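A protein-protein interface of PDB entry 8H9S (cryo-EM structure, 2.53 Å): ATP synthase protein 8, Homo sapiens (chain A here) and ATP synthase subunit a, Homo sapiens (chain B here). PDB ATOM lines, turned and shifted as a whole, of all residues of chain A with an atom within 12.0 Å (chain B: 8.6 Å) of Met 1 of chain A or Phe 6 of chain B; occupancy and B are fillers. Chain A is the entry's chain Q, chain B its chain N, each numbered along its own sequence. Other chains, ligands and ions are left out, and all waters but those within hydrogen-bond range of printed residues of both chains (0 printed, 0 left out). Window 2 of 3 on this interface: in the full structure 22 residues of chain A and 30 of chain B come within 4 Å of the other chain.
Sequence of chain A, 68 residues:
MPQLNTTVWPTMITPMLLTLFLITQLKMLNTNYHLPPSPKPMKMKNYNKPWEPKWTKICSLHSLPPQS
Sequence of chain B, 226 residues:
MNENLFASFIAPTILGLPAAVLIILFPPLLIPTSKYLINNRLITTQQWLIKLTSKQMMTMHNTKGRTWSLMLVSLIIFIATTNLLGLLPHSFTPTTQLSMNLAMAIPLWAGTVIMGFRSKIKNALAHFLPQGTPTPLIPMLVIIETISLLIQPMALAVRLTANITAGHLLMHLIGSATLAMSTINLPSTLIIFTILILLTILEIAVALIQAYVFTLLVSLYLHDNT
The side-chain hydroxyl (OG1) of Thr 96 of chain B lies within hydrogen-bond range of the side-chain amide nitrogen (NE2) of Gln 97 of chain B, at 3.2 Å. O of Thr 161 of chain B lies within hydrogen-bond range of OG1 of Thr 165 of chain B, at 3.0 Å. NE2 of Gln 97 of chain B sits at hydrogen-bond distance from O of Phe 9 of chain B. O of Gln 3 of chain A lies within hydrogen-bond range of NE1 of Trp 9 of chain A (3.2 Å). The backbone carbonyl oxygen of Thr 96 of chain B sits at hydrogen-bond distance from the side-chain hydroxyl of Thr 165 of chain B (3.3 Å).
Met 1 of chain A touches one residue of chain B. Pro 2 of chain A touches just these residues of chain B: Phe 6, Phe 9 and Ile 10. Printed residues of chain B within 4 Å of Gln 3 of chain A: Phe 9 (3.9 Å), Thr 96 (3.0 Å), Gln 97 (3.9 Å) and Thr 165 (3.5 Å). Printed residues of chain B within 4 Å of Met 12 of chain A: Ala 11 (3.5 Å) and Phe 92 (3.5 Å). No residue of chain A comes within 4 Å of Asn 4 of chain B. No residue of chain A comes within 4 Å of Leu 5 of chain B. Of the printed residues of chain A, Phe 6 of chain B touches Met 1 (3.5 Å) and Pro 2 (3.5 Å). No residue of chain A comes within 4 Å of Ala 7 of chain B. Phe 9 of chain B touches just these residues of chain A: Pro 2 and Gln 3. Of the printed residues of chain A, Ile 10 of chain B touches Pro 2 (3.6 Å). Printed residues of chain A within 4 Å of Thr 96 of chain B: Gln 3. Of the printed residues of chain A, Thr 165 of chain B touches Gln 3. The nearest residue of chain B that does not touch Met 1 of chain A is Thr 165 of chain B (5.1 Å). The nearest printed residue of chain A that does not touch Gln 97 of chain B is Met 12 of chain A (4.3 Å).
Hydrophobic or aromatic side chains of chain A within 4 Å of the printed part of chain B: Met 1, Pro 2 and Met 12. Among the printed residues, 10 pairs touch across the chains.
Among the printed residues, merely in contact across the chains: Met 1 of chain A with Phe 6 of chain B, Pro 2 of chain A with Phe 6 of chain B, Pro 2 of chain A with Phe 9 of chain B, Pro 2 of chain A with Ile 10 of chain B, Gln 3 of chain A with Phe 9 of chain B, Gln 3 of chain A with Gln 97 of chain B, Gln 3 of chain A with Thr 165 of chain B, Met 12 of chain A with Ala 11 of chain B and Met 12 of chain A with Phe 92 of chain B.
NE2 of Gln 3 of chain A sits at hydrogen-bond distance from O of Thr 96 of chain B, at 3.0 Å.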
ATOM      1  N   MET A   1       4.719  24.431 -16.503  1.00  0.00           N
ATOM      2  CA  MET A   1       4.425  23.195 -15.791  1.00  0.00           C
ATOM      3  C   MET A   1       5.408  22.103 -16.174  1.00  0.00           C
ATOM      4  O   MET A   1       5.496  21.728 -17.340  1.00  0.00           O
ATOM      5  CB  MET A   1       3.001  22.726 -16.080  1.00  0.00           C
ATOM      6  CG  MET A   1       1.946  23.798 -15.938  1.00  0.00           C
ATOM      7  SD  MET A   1       1.668  24.259 -14.227  1.00  0.00           S
ATOM      8  CE  MET A   1       0.730  22.850 -13.653  1.00  0.00           C
ATOM      9  N   PRO A   2       6.152  21.591 -15.194  1.00  0.00           N
ATOM     10  CA  PRO A   2       7.047  20.459 -15.474  1.00  0.00           C
ATOM     11  C   PRO A   2       6.318  19.203 -15.907  1.00  0.00           C
ATOM     12  O   PRO A   2       6.956  18.291 -16.443  1.00  0.00           O
ATOM     13  CB  PRO A   2       7.782  20.251 -14.144  1.00  0.00           C
ATOM     14  CG  PRO A   2       7.002  21.010 -13.131  1.00  0.00           C
ATOM     15  CD  PRO A   2       6.351  22.133 -13.843  1.00  0.00           C
ATOM     16  N   GLN A   3       5.005  19.120 -15.693  1.00  0.00           N
ATOM     17  CA  GLN A   3       4.246  17.972 -16.168  1.00  0.00           C
ATOM     18  C   GLN A   3       4.084  17.973 -17.678  1.00  0.00           C
ATOM     19  O   GLN A   3       3.709  16.946 -18.248  1.00  0.00           O
ATOM     20  CB  GLN A   3       2.869  17.943 -15.514  1.00  0.00           C
ATOM     21  CG  GLN A   3       2.885  17.569 -14.059  1.00  0.00           C
ATOM     22  CD  GLN A   3       2.975  18.765 -13.153  1.00  0.00           C
ATOM     23  OE1 GLN A   3       3.717  19.704 -13.419  1.00  0.00           O
ATOM     24  NE2 GLN A   3       2.219  18.739 -12.070  1.00  0.00           N
ATOM     25  N   LEU A   4       4.345  19.100 -18.335  1.00  0.00           N
ATOM     26  CA  LEU A   4       4.215  19.202 -19.779  1.00  0.00           C
ATOM     27  C   LEU A   4       5.531  18.985 -20.509  1.00  0.00           C
ATOM     28  O   LEU A   4       5.529  18.890 -21.738  1.00  0.00           O
ATOM     29  CB  LEU A   4       3.635  20.566 -20.162  1.00  0.00           C
ATOM     30  CG  LEU A   4       2.209  20.812 -19.672  1.00  0.00           C
ATOM     31  CD1 LEU A   4       1.735  22.182 -20.088  1.00  0.00           C
ATOM     32  CD2 LEU A   4       1.275  19.748 -20.201  1.00  0.00           C
ATOM     33  N   ASN A   5       6.641  18.899 -19.788  1.00  0.00           N
ATOM     34  CA  ASN A   5       7.930  18.563 -20.382  1.00  0.00           C
ATOM     35  C   ASN A   5       7.896  17.095 -20.777  1.00  0.00           C
ATOM     36  O   ASN A   5       8.098  16.212 -19.946  1.00  0.00           O
ATOM     37  CB  ASN A   5       9.052  18.850 -19.393  1.00  0.00           C
ATOM     38  CG  ASN A   5      10.395  18.348 -19.865  1.00  0.00           C
ATOM     39  OD1 ASN A   5      10.595  18.085 -21.048  1.00  0.00           O
ATOM     40  ND2 ASN A   5      11.331  18.219 -18.937  1.00  0.00           N
ATOM     41  N   THR A   6       7.642  16.830 -22.057  1.00  0.00           N
ATOM     42  CA  THR A   6       7.463  15.472 -22.550  1.00  0.00           C
ATOM     43  C   THR A   6       8.767  14.701 -22.691  1.00  0.00           C
ATOM     44  O   THR A   6       8.749  13.583 -23.210  1.00  0.00           O
ATOM     45  CB  THR A   6       6.746  15.491 -23.899  1.00  0.00           C
ATOM     46  OG1 THR A   6       7.526  16.236 -24.840  1.00  0.00           O
ATOM     47  CG2 THR A   6       5.389  16.137 -23.766  1.00  0.00           C
ATOM     48  N   THR A   7       9.890  15.259 -22.249  1.00  0.00           N
ATOM     49  CA  THR A   7      11.159  14.557 -22.377  1.00  0.00           C
ATOM     50  C   THR A   7      11.330  13.499 -21.298  1.00  0.00           C
ATOM     51  O   THR A   7      11.949  12.459 -21.544  1.00  0.00           O
ATOM     52  CB  THR A   7      12.311  15.559 -22.333  1.00  0.00           C
ATOM     53  OG1 THR A   7      12.169  16.486 -23.414  1.00  0.00           O
ATOM     54  CG2 THR A   7      13.645  14.859 -22.467  1.00  0.00           C
ATOM     55  N   VAL A   8      10.775  13.729 -20.114  1.00  0.00           N
ATOM     56  CA  VAL A   8      10.877  12.785 -19.015  1.00  0.00           C
ATOM     57  C   VAL A   8       9.619  11.925 -18.898  1.00  0.00           C
ATOM     58  O   VAL A   8       9.359  11.354 -17.844  1.00  0.00           O
ATOM     59  CB  VAL A   8      11.186  13.494 -17.691  1.00  0.00           C
ATOM     60  CG1 VAL A   8      12.471  14.279 -17.805  1.00  0.00           C
ATOM     61  CG2 VAL A   8      10.048  14.410 -17.311  1.00  0.00           C
ATOM     62  N   TRP A   9       8.836  11.821 -19.964  1.00  0.00           N
ATOM     63  CA  TRP A   9       7.594  11.067 -19.900  1.00  0.00           C
ATOM     64  C   TRP A   9       7.827   9.559 -19.880  1.00  0.00           C
ATOM     65  O   TRP A   9       7.121   8.858 -19.149  1.00  0.00           O
ATOM     66  CB  TRP A   9       6.673  11.447 -21.057  1.00  0.00           C
ATOM     67  CG  TRP A   9       5.773  12.591 -20.730  1.00  0.00           C
ATOM     68  CD1 TRP A   9       6.022  13.598 -19.850  1.00  0.00           C
ATOM     69  CD2 TRP A   9       4.473  12.842 -21.269  1.00  0.00           C
ATOM     70  NE1 TRP A   9       4.963  14.465 -19.812  1.00  0.00           N
ATOM     71  CE2 TRP A   9       3.998  14.023 -20.676  1.00  0.00           C
ATOM     72  CE3 TRP A   9       3.667  12.184 -22.199  1.00  0.00           C
ATOM     73  CZ2 TRP A   9       2.755  14.559 -20.978  1.00  0.00           C
ATOM     74  CZ3 TRP A   9       2.434  12.719 -22.498  1.00  0.00           C
ATOM     75  CH2 TRP A   9       1.988  13.892 -21.890  1.00  0.00           C
ATOM     76  N   MET A  12       8.704   8.248 -16.420  1.00  0.00           N
ATOM     77  CA  MET A  12       7.568   8.144 -15.516  1.00  0.00           C
ATOM     78  C   MET A  12       6.597   7.045 -15.899  1.00  0.00           C
ATOM     79  O   MET A  12       5.800   6.628 -15.056  1.00  0.00           O
ATOM     80  CB  MET A  12       6.800   9.464 -15.465  1.00  0.00           C
ATOM     81  CG  MET A  12       7.627  10.645 -15.059  1.00  0.00           C
ATOM     82  SD  MET A  12       8.117  10.556 -13.344  1.00  0.00           S
ATOM     83  CE  MET A  12       9.336  11.853 -13.334  1.00  0.00           C
ATOM     84  N   ASN B   4      10.801  27.043  -9.334  1.00  0.00           N
ATOM     85  CA  ASN B   4      10.720  27.843  -8.120  1.00  0.00           C
ATOM     86  C   ASN B   4       9.516  27.441  -7.270  1.00  0.00           C
ATOM     87  O   ASN B   4       9.654  27.144  -6.084  1.00  0.00           O
ATOM     88  CB  ASN B   4      10.661  29.332  -8.468  1.00  0.00           C
ATOM     89  CG  ASN B   4       9.589  29.650  -9.495  1.00  0.00           C
ATOM     90  OD1 ASN B   4       8.864  28.765  -9.947  1.00  0.00           O
ATOM     91  ND2 ASN B   4       9.480  30.921  -9.864  1.00  0.00           N
ATOM     92  N   LEU B   5       8.337  27.432  -7.885  1.00  0.00           N
ATOM     93  CA  LEU B   5       7.107  27.012  -7.228  1.00  0.00           C
ATOM     94  C   LEU B   5       6.726  25.582  -7.568  1.00  0.00           C
ATOM     95  O   LEU B   5       6.230  24.853  -6.706  1.00  0.00           O
ATOM     96  CB  LEU B   5       5.958  27.949  -7.614  1.00  0.00           C
ATOM     97  CG  LEU B   5       4.587  27.638  -7.017  1.00  0.00           C
ATOM     98  CD1 LEU B   5       4.562  27.990  -5.544  1.00  0.00           C
ATOM     99  CD2 LEU B   5       3.500  28.377  -7.769  1.00  0.00           C
ATOM    100  N   PHE B   6       6.950  25.168  -8.813  1.00  0.00           N
ATOM    101  CA  PHE B   6       6.723  23.798  -9.249  1.00  0.00           C
ATOM    102  C   PHE B   6       7.978  22.950  -9.159  1.00  0.00           C
ATOM    103  O   PHE B   6       8.133  22.000  -9.931  1.00  0.00           O
ATOM    104  CB  PHE B   6       6.181  23.785 -10.676  1.00  0.00           C
ATOM    105  CG  PHE B   6       4.838  24.429 -10.816  1.00  0.00           C
ATOM    106  CD1 PHE B   6       4.728  25.784 -11.050  1.00  0.00           C
ATOM    107  CD2 PHE B   6       3.685  23.677 -10.716  1.00  0.00           C
ATOM    108  CE1 PHE B   6       3.495  26.375 -11.176  1.00  0.00           C
ATOM    109  CE2 PHE B   6       2.449  24.265 -10.842  1.00  0.00           C
ATOM    110  CZ  PHE B   6       2.355  25.615 -11.072  1.00  0.00           C
ATOM    111  N   ALA B   7       8.887  23.275  -8.243  1.00  0.00           N
ATOM    112  CA  ALA B   7      10.118  22.511  -8.116  1.00  0.00           C
ATOM    113  C   ALA B   7       9.875  21.103  -7.601  1.00  0.00           C
ATOM    114  O   ALA B   7      10.696  20.218  -7.851  1.00  0.00           O
ATOM    115  CB  ALA B   7      11.093  23.238  -7.194  1.00  0.00           C
ATOM    116  N   SER B   8       8.772  20.875  -6.894  1.00  0.00           N
ATOM    117  CA  SER B   8       8.471  19.563  -6.343  1.00  0.00           C
ATOM    118  C   SER B   8       7.809  18.634  -7.347  1.00  0.00           C
ATOM    119  O   SER B   8       7.548  17.476  -7.012  1.00  0.00           O
ATOM    120  CB  SER B   8       7.574  19.705  -5.115  1.00  0.00           C
ATOM    121  OG  SER B   8       8.189  20.519  -4.135  1.00  0.00           O
ATOM    122  N   PHE B   9       7.524  19.111  -8.556  1.00  0.00           N
ATOM    123  CA  PHE B   9       6.918  18.301  -9.601  1.00  0.00           C
ATOM    124  C   PHE B   9       7.884  18.023 -10.741  1.00  0.00           C
ATOM    125  O   PHE B   9       7.480  17.454 -11.759  1.00  0.00           O
ATOM    126  CB  PHE B   9       5.654  18.977 -10.131  1.00  0.00           C
ATOM    127  CG  PHE B   9       4.735  19.460  -9.053  1.00  0.00           C
ATOM    128  CD1 PHE B   9       4.566  20.806  -8.825  1.00  0.00           C
ATOM    129  CD2 PHE B   9       4.049  18.570  -8.262  1.00  0.00           C
ATOM    130  CE1 PHE B   9       3.731  21.251  -7.831  1.00  0.00           C
ATOM    131  CE2 PHE B   9       3.213  19.015  -7.267  1.00  0.00           C
ATOM    132  CZ  PHE B   9       3.056  20.357  -7.055  1.00  0.00           C
ATOM    133  N   ILE B  10       9.138  18.408 -10.596  1.00  0.00           N
ATOM    134  CA  ILE B  10      10.163  18.151 -11.596  1.00  0.00           C
ATOM    135  C   ILE B  10      10.781  16.794 -11.315  1.00  0.00           C
ATOM    136  O   ILE B  10      11.059  16.455 -10.160  1.00  0.00           O
ATOM    137  CB  ILE B  10      11.231  19.257 -11.584  1.00  0.00           C
ATOM    138  CG1 ILE B  10      10.604  20.611 -11.900  1.00  0.00           C
ATOM    139  CG2 ILE B  10      12.325  18.953 -12.582  1.00  0.00           C
ATOM    140  CD1 ILE B  10      11.550  21.763 -11.710  1.00  0.00           C
ATOM    141  N   ALA B  11      10.990  16.012 -12.374  1.00  0.00           N
ATOM    142  CA  ALA B  11      11.591  14.687 -12.302  1.00  0.00           C
ATOM    143  C   ALA B  11      12.849  14.717 -11.448  1.00  0.00           C
ATOM    144  O   ALA B  11      13.851  15.328 -11.839  1.00  0.00           O
ATOM    145  CB  ALA B  11      11.920  14.174 -13.700  1.00  0.00           C
ATOM    146  N   PHE B  92       8.670  13.332  -3.834  1.00  0.00           N
ATOM    147  CA  PHE B  92       8.195  13.490  -5.199  1.00  0.00           C
ATOM    148  C   PHE B  92       7.033  12.531  -5.402  1.00  0.00           C
ATOM    149  O   PHE B  92       7.181  11.323  -5.195  1.00  0.00           O
ATOM    150  CB  PHE B  92       9.317  13.217  -6.197  1.00  0.00           C
ATOM    151  CG  PHE B  92       8.850  13.057  -7.611  1.00  0.00           C
ATOM    152  CD1 PHE B  92       8.507  14.157  -8.366  1.00  0.00           C
ATOM    153  CD2 PHE B  92       8.768  11.806  -8.190  1.00  0.00           C
ATOM    154  CE1 PHE B  92       8.082  14.011  -9.660  1.00  0.00           C
ATOM    155  CE2 PHE B  92       8.344  11.659  -9.487  1.00  0.00           C
ATOM    156  CZ  PHE B  92       8.001  12.762 -10.220  1.00  0.00           C
ATOM    157  N   THR B  96       1.281  13.209  -9.451  1.00  0.00           N
ATOM    158  CA  THR B  96       1.158  14.588  -9.894  1.00  0.00           C
ATOM    159  C   THR B  96       1.556  14.765 -11.347  1.00  0.00           C
ATOM    160  O   THR B  96       1.475  15.884 -11.856  1.00  0.00           O
ATOM    161  CB  THR B  96       2.017  15.515  -9.036  1.00  0.00           C
ATOM    162  OG1 THR B  96       3.399  15.236  -9.267  1.00  0.00           O
ATOM    163  CG2 THR B  96       1.722  15.318  -7.580  1.00  0.00           C
ATOM    164  N   GLN B  97       1.979  13.700 -12.017  1.00  0.00           N
ATOM    165  CA  GLN B  97       2.471  13.765 -13.384  1.00  0.00           C
ATOM    166  C   GLN B  97       1.383  13.314 -14.345  1.00  0.00           C
ATOM    167  O   GLN B  97       0.770  12.264 -14.143  1.00  0.00           O
ATOM    168  CB  GLN B  97       3.710  12.890 -13.552  1.00  0.00           C
ATOM    169  CG  GLN B  97       4.749  13.091 -12.484  1.00  0.00           C
ATOM    170  CD  GLN B  97       5.521  14.366 -12.669  1.00  0.00           C
ATOM    171  OE1 GLN B  97       6.041  14.637 -13.747  1.00  0.00           O
ATOM    172  NE2 GLN B  97       5.602  15.163 -11.617  1.00  0.00           N
ATOM    173  N   LEU B  98       1.154  14.103 -15.391  1.00  0.00           N
ATOM    174  CA  LEU B  98       0.133  13.754 -16.367  1.00  0.00           C
ATOM    175  C   LEU B  98       0.526  12.542 -17.194  1.00  0.00           C
ATOM    176  O   LEU B  98      -0.354  11.835 -17.691  1.00  0.00           O
ATOM    177  CB  LEU B  98      -0.146  14.953 -17.274  1.00  0.00           C
ATOM    178  CG  LEU B  98      -1.207  14.831 -18.367  1.00  0.00           C
ATOM    179  CD1 LEU B  98      -2.580  14.610 -17.780  1.00  0.00           C
ATOM    180  CD2 LEU B  98      -1.194  16.069 -19.232  1.00  0.00           C
ATOM    181  N   THR B 161      -4.439  13.984 -11.657  1.00  0.00           N
ATOM    182  CA  THR B 161      -3.320  14.918 -11.681  1.00  0.00           C
ATOM    183  C   THR B 161      -3.725  16.251 -11.081  1.00  0.00           C
ATOM    184  O   THR B 161      -3.264  16.629  -9.997  1.00  0.00           O
ATOM    185  CB  THR B 161      -2.838  15.110 -13.117  1.00  0.00           C
ATOM    186  OG1 THR B 161      -2.592  13.835 -13.714  1.00  0.00           O
ATOM    187  CG2 THR B 161      -1.570  15.924 -13.146  1.00  0.00           C
ATOM    188  N   ALA B 162      -4.660  16.933 -11.745  1.00  0.00           N
ATOM    189  CA  ALA B 162      -5.128  18.236 -11.302  1.00  0.00           C
ATOM    190  C   ALA B 162      -5.479  18.245  -9.829  1.00  0.00           C
ATOM    191  O   ALA B 162      -5.361  19.281  -9.176  1.00  0.00           O
ATOM    192  CB  ALA B 162      -6.338  18.665 -12.127  1.00  0.00           C
ATOM    193  N   THR B 165      -1.645  17.352  -7.548  1.00  0.00           N
ATOM    194  CA  THR B 165      -0.867  18.564  -7.759  1.00  0.00           C
ATOM    195  C   THR B 165      -1.427  19.721  -6.955  1.00  0.00           C
ATOM    196  O   THR B 165      -0.753  20.260  -6.070  1.00  0.00           O
ATOM    197  CB  THR B 165      -0.856  18.924  -9.243  1.00  0.00           C
ATOM    198  OG1 THR B 165      -0.507  17.774 -10.015  1.00  0.00           O
ATOM    199  CG2 THR B 165       0.144  20.018  -9.507  1.00  0.00           C
ATOM    200  N   ALA B 166      -2.694  20.060  -7.205  1.00  0.00           N
ATOM    201  CA  ALA B 166      -3.289  21.221  -6.558  1.00  0.00           C
ATOM    202  C   ALA B 166      -3.127  21.135  -5.054  1.00  0.00           C
ATOM    203  O   ALA B 166      -2.601  22.059  -4.422  1.00  0.00           O
ATOM    204  CB  ALA B 166      -4.761  21.341  -6.935  1.00  0.00           C
ATOM    205  N   LEU B 169       0.367  21.896  -4.020  1.00  0.00           N
ATOM    206  CA  LEU B 169       0.601  23.323  -4.181  1.00  0.00           C
ATOM    207  C   LEU B 169       0.045  24.086  -2.995  1.00  0.00           C
ATOM    208  O   LEU B 169       0.776  24.803  -2.302  1.00  0.00           O
ATOM    209  CB  LEU B 169      -0.028  23.820  -5.479  1.00  0.00           C
ATOM    210  CG  LEU B 169       0.917  23.958  -6.664  1.00  0.00           C
ATOM    211  CD1 LEU B 169       0.133  24.088  -7.947  1.00  0.00           C
ATOM    212  CD2 LEU B 169       1.807  25.156  -6.463  1.00  0.00           C
ATOM    213  N   HIS B 172       2.074  23.674   0.155  1.00  0.00           N
ATOM    214  CA  HIS B 172       3.338  24.390   0.065  1.00  0.00           C
ATOM    215  C   HIS B 172       3.121  25.873   0.289  1.00  0.00           C
ATOM    216  O   HIS B 172       3.801  26.494   1.112  1.00  0.00           O
ATOM    217  CB  HIS B 172       3.995  24.143  -1.289  1.00  0.00           C
ATOM    218  CG  HIS B 172       5.319  24.822  -1.445  1.00  0.00           C
ATOM    219  ND1 HIS B 172       5.503  25.918  -2.257  1.00  0.00           N
ATOM    220  CD2 HIS B 172       6.524  24.561  -0.887  1.00  0.00           C
ATOM    221  CE1 HIS B 172       6.764  26.304  -2.194  1.00  0.00           C
ATOM    222  NE2 HIS B 172       7.406  25.497  -1.370  1.00  0.00           N
ATOM    223  N   LEU B 173       2.122  26.443  -0.387  1.00  0.00           N
ATOM    224  CA  LEU B 173       1.872  27.870  -0.242  1.00  0.00           C
ATOM    225  C   LEU B 173       1.592  28.219   1.208  1.00  0.00           C
ATOM    226  O   LEU B 173       2.212  29.130   1.768  1.00  0.00           O
ATOM    227  CB  LEU B 173       0.719  28.297  -1.145  1.00  0.00           C
ATOM    228  CG  LEU B 173       1.115  28.379  -2.617  1.00  0.00           C
ATOM    229  CD1 LEU B 173       0.038  29.064  -3.415  1.00  0.00           C
ATOM    230  CD2 LEU B 173       2.428  29.110  -2.766  1.00  0.00           C
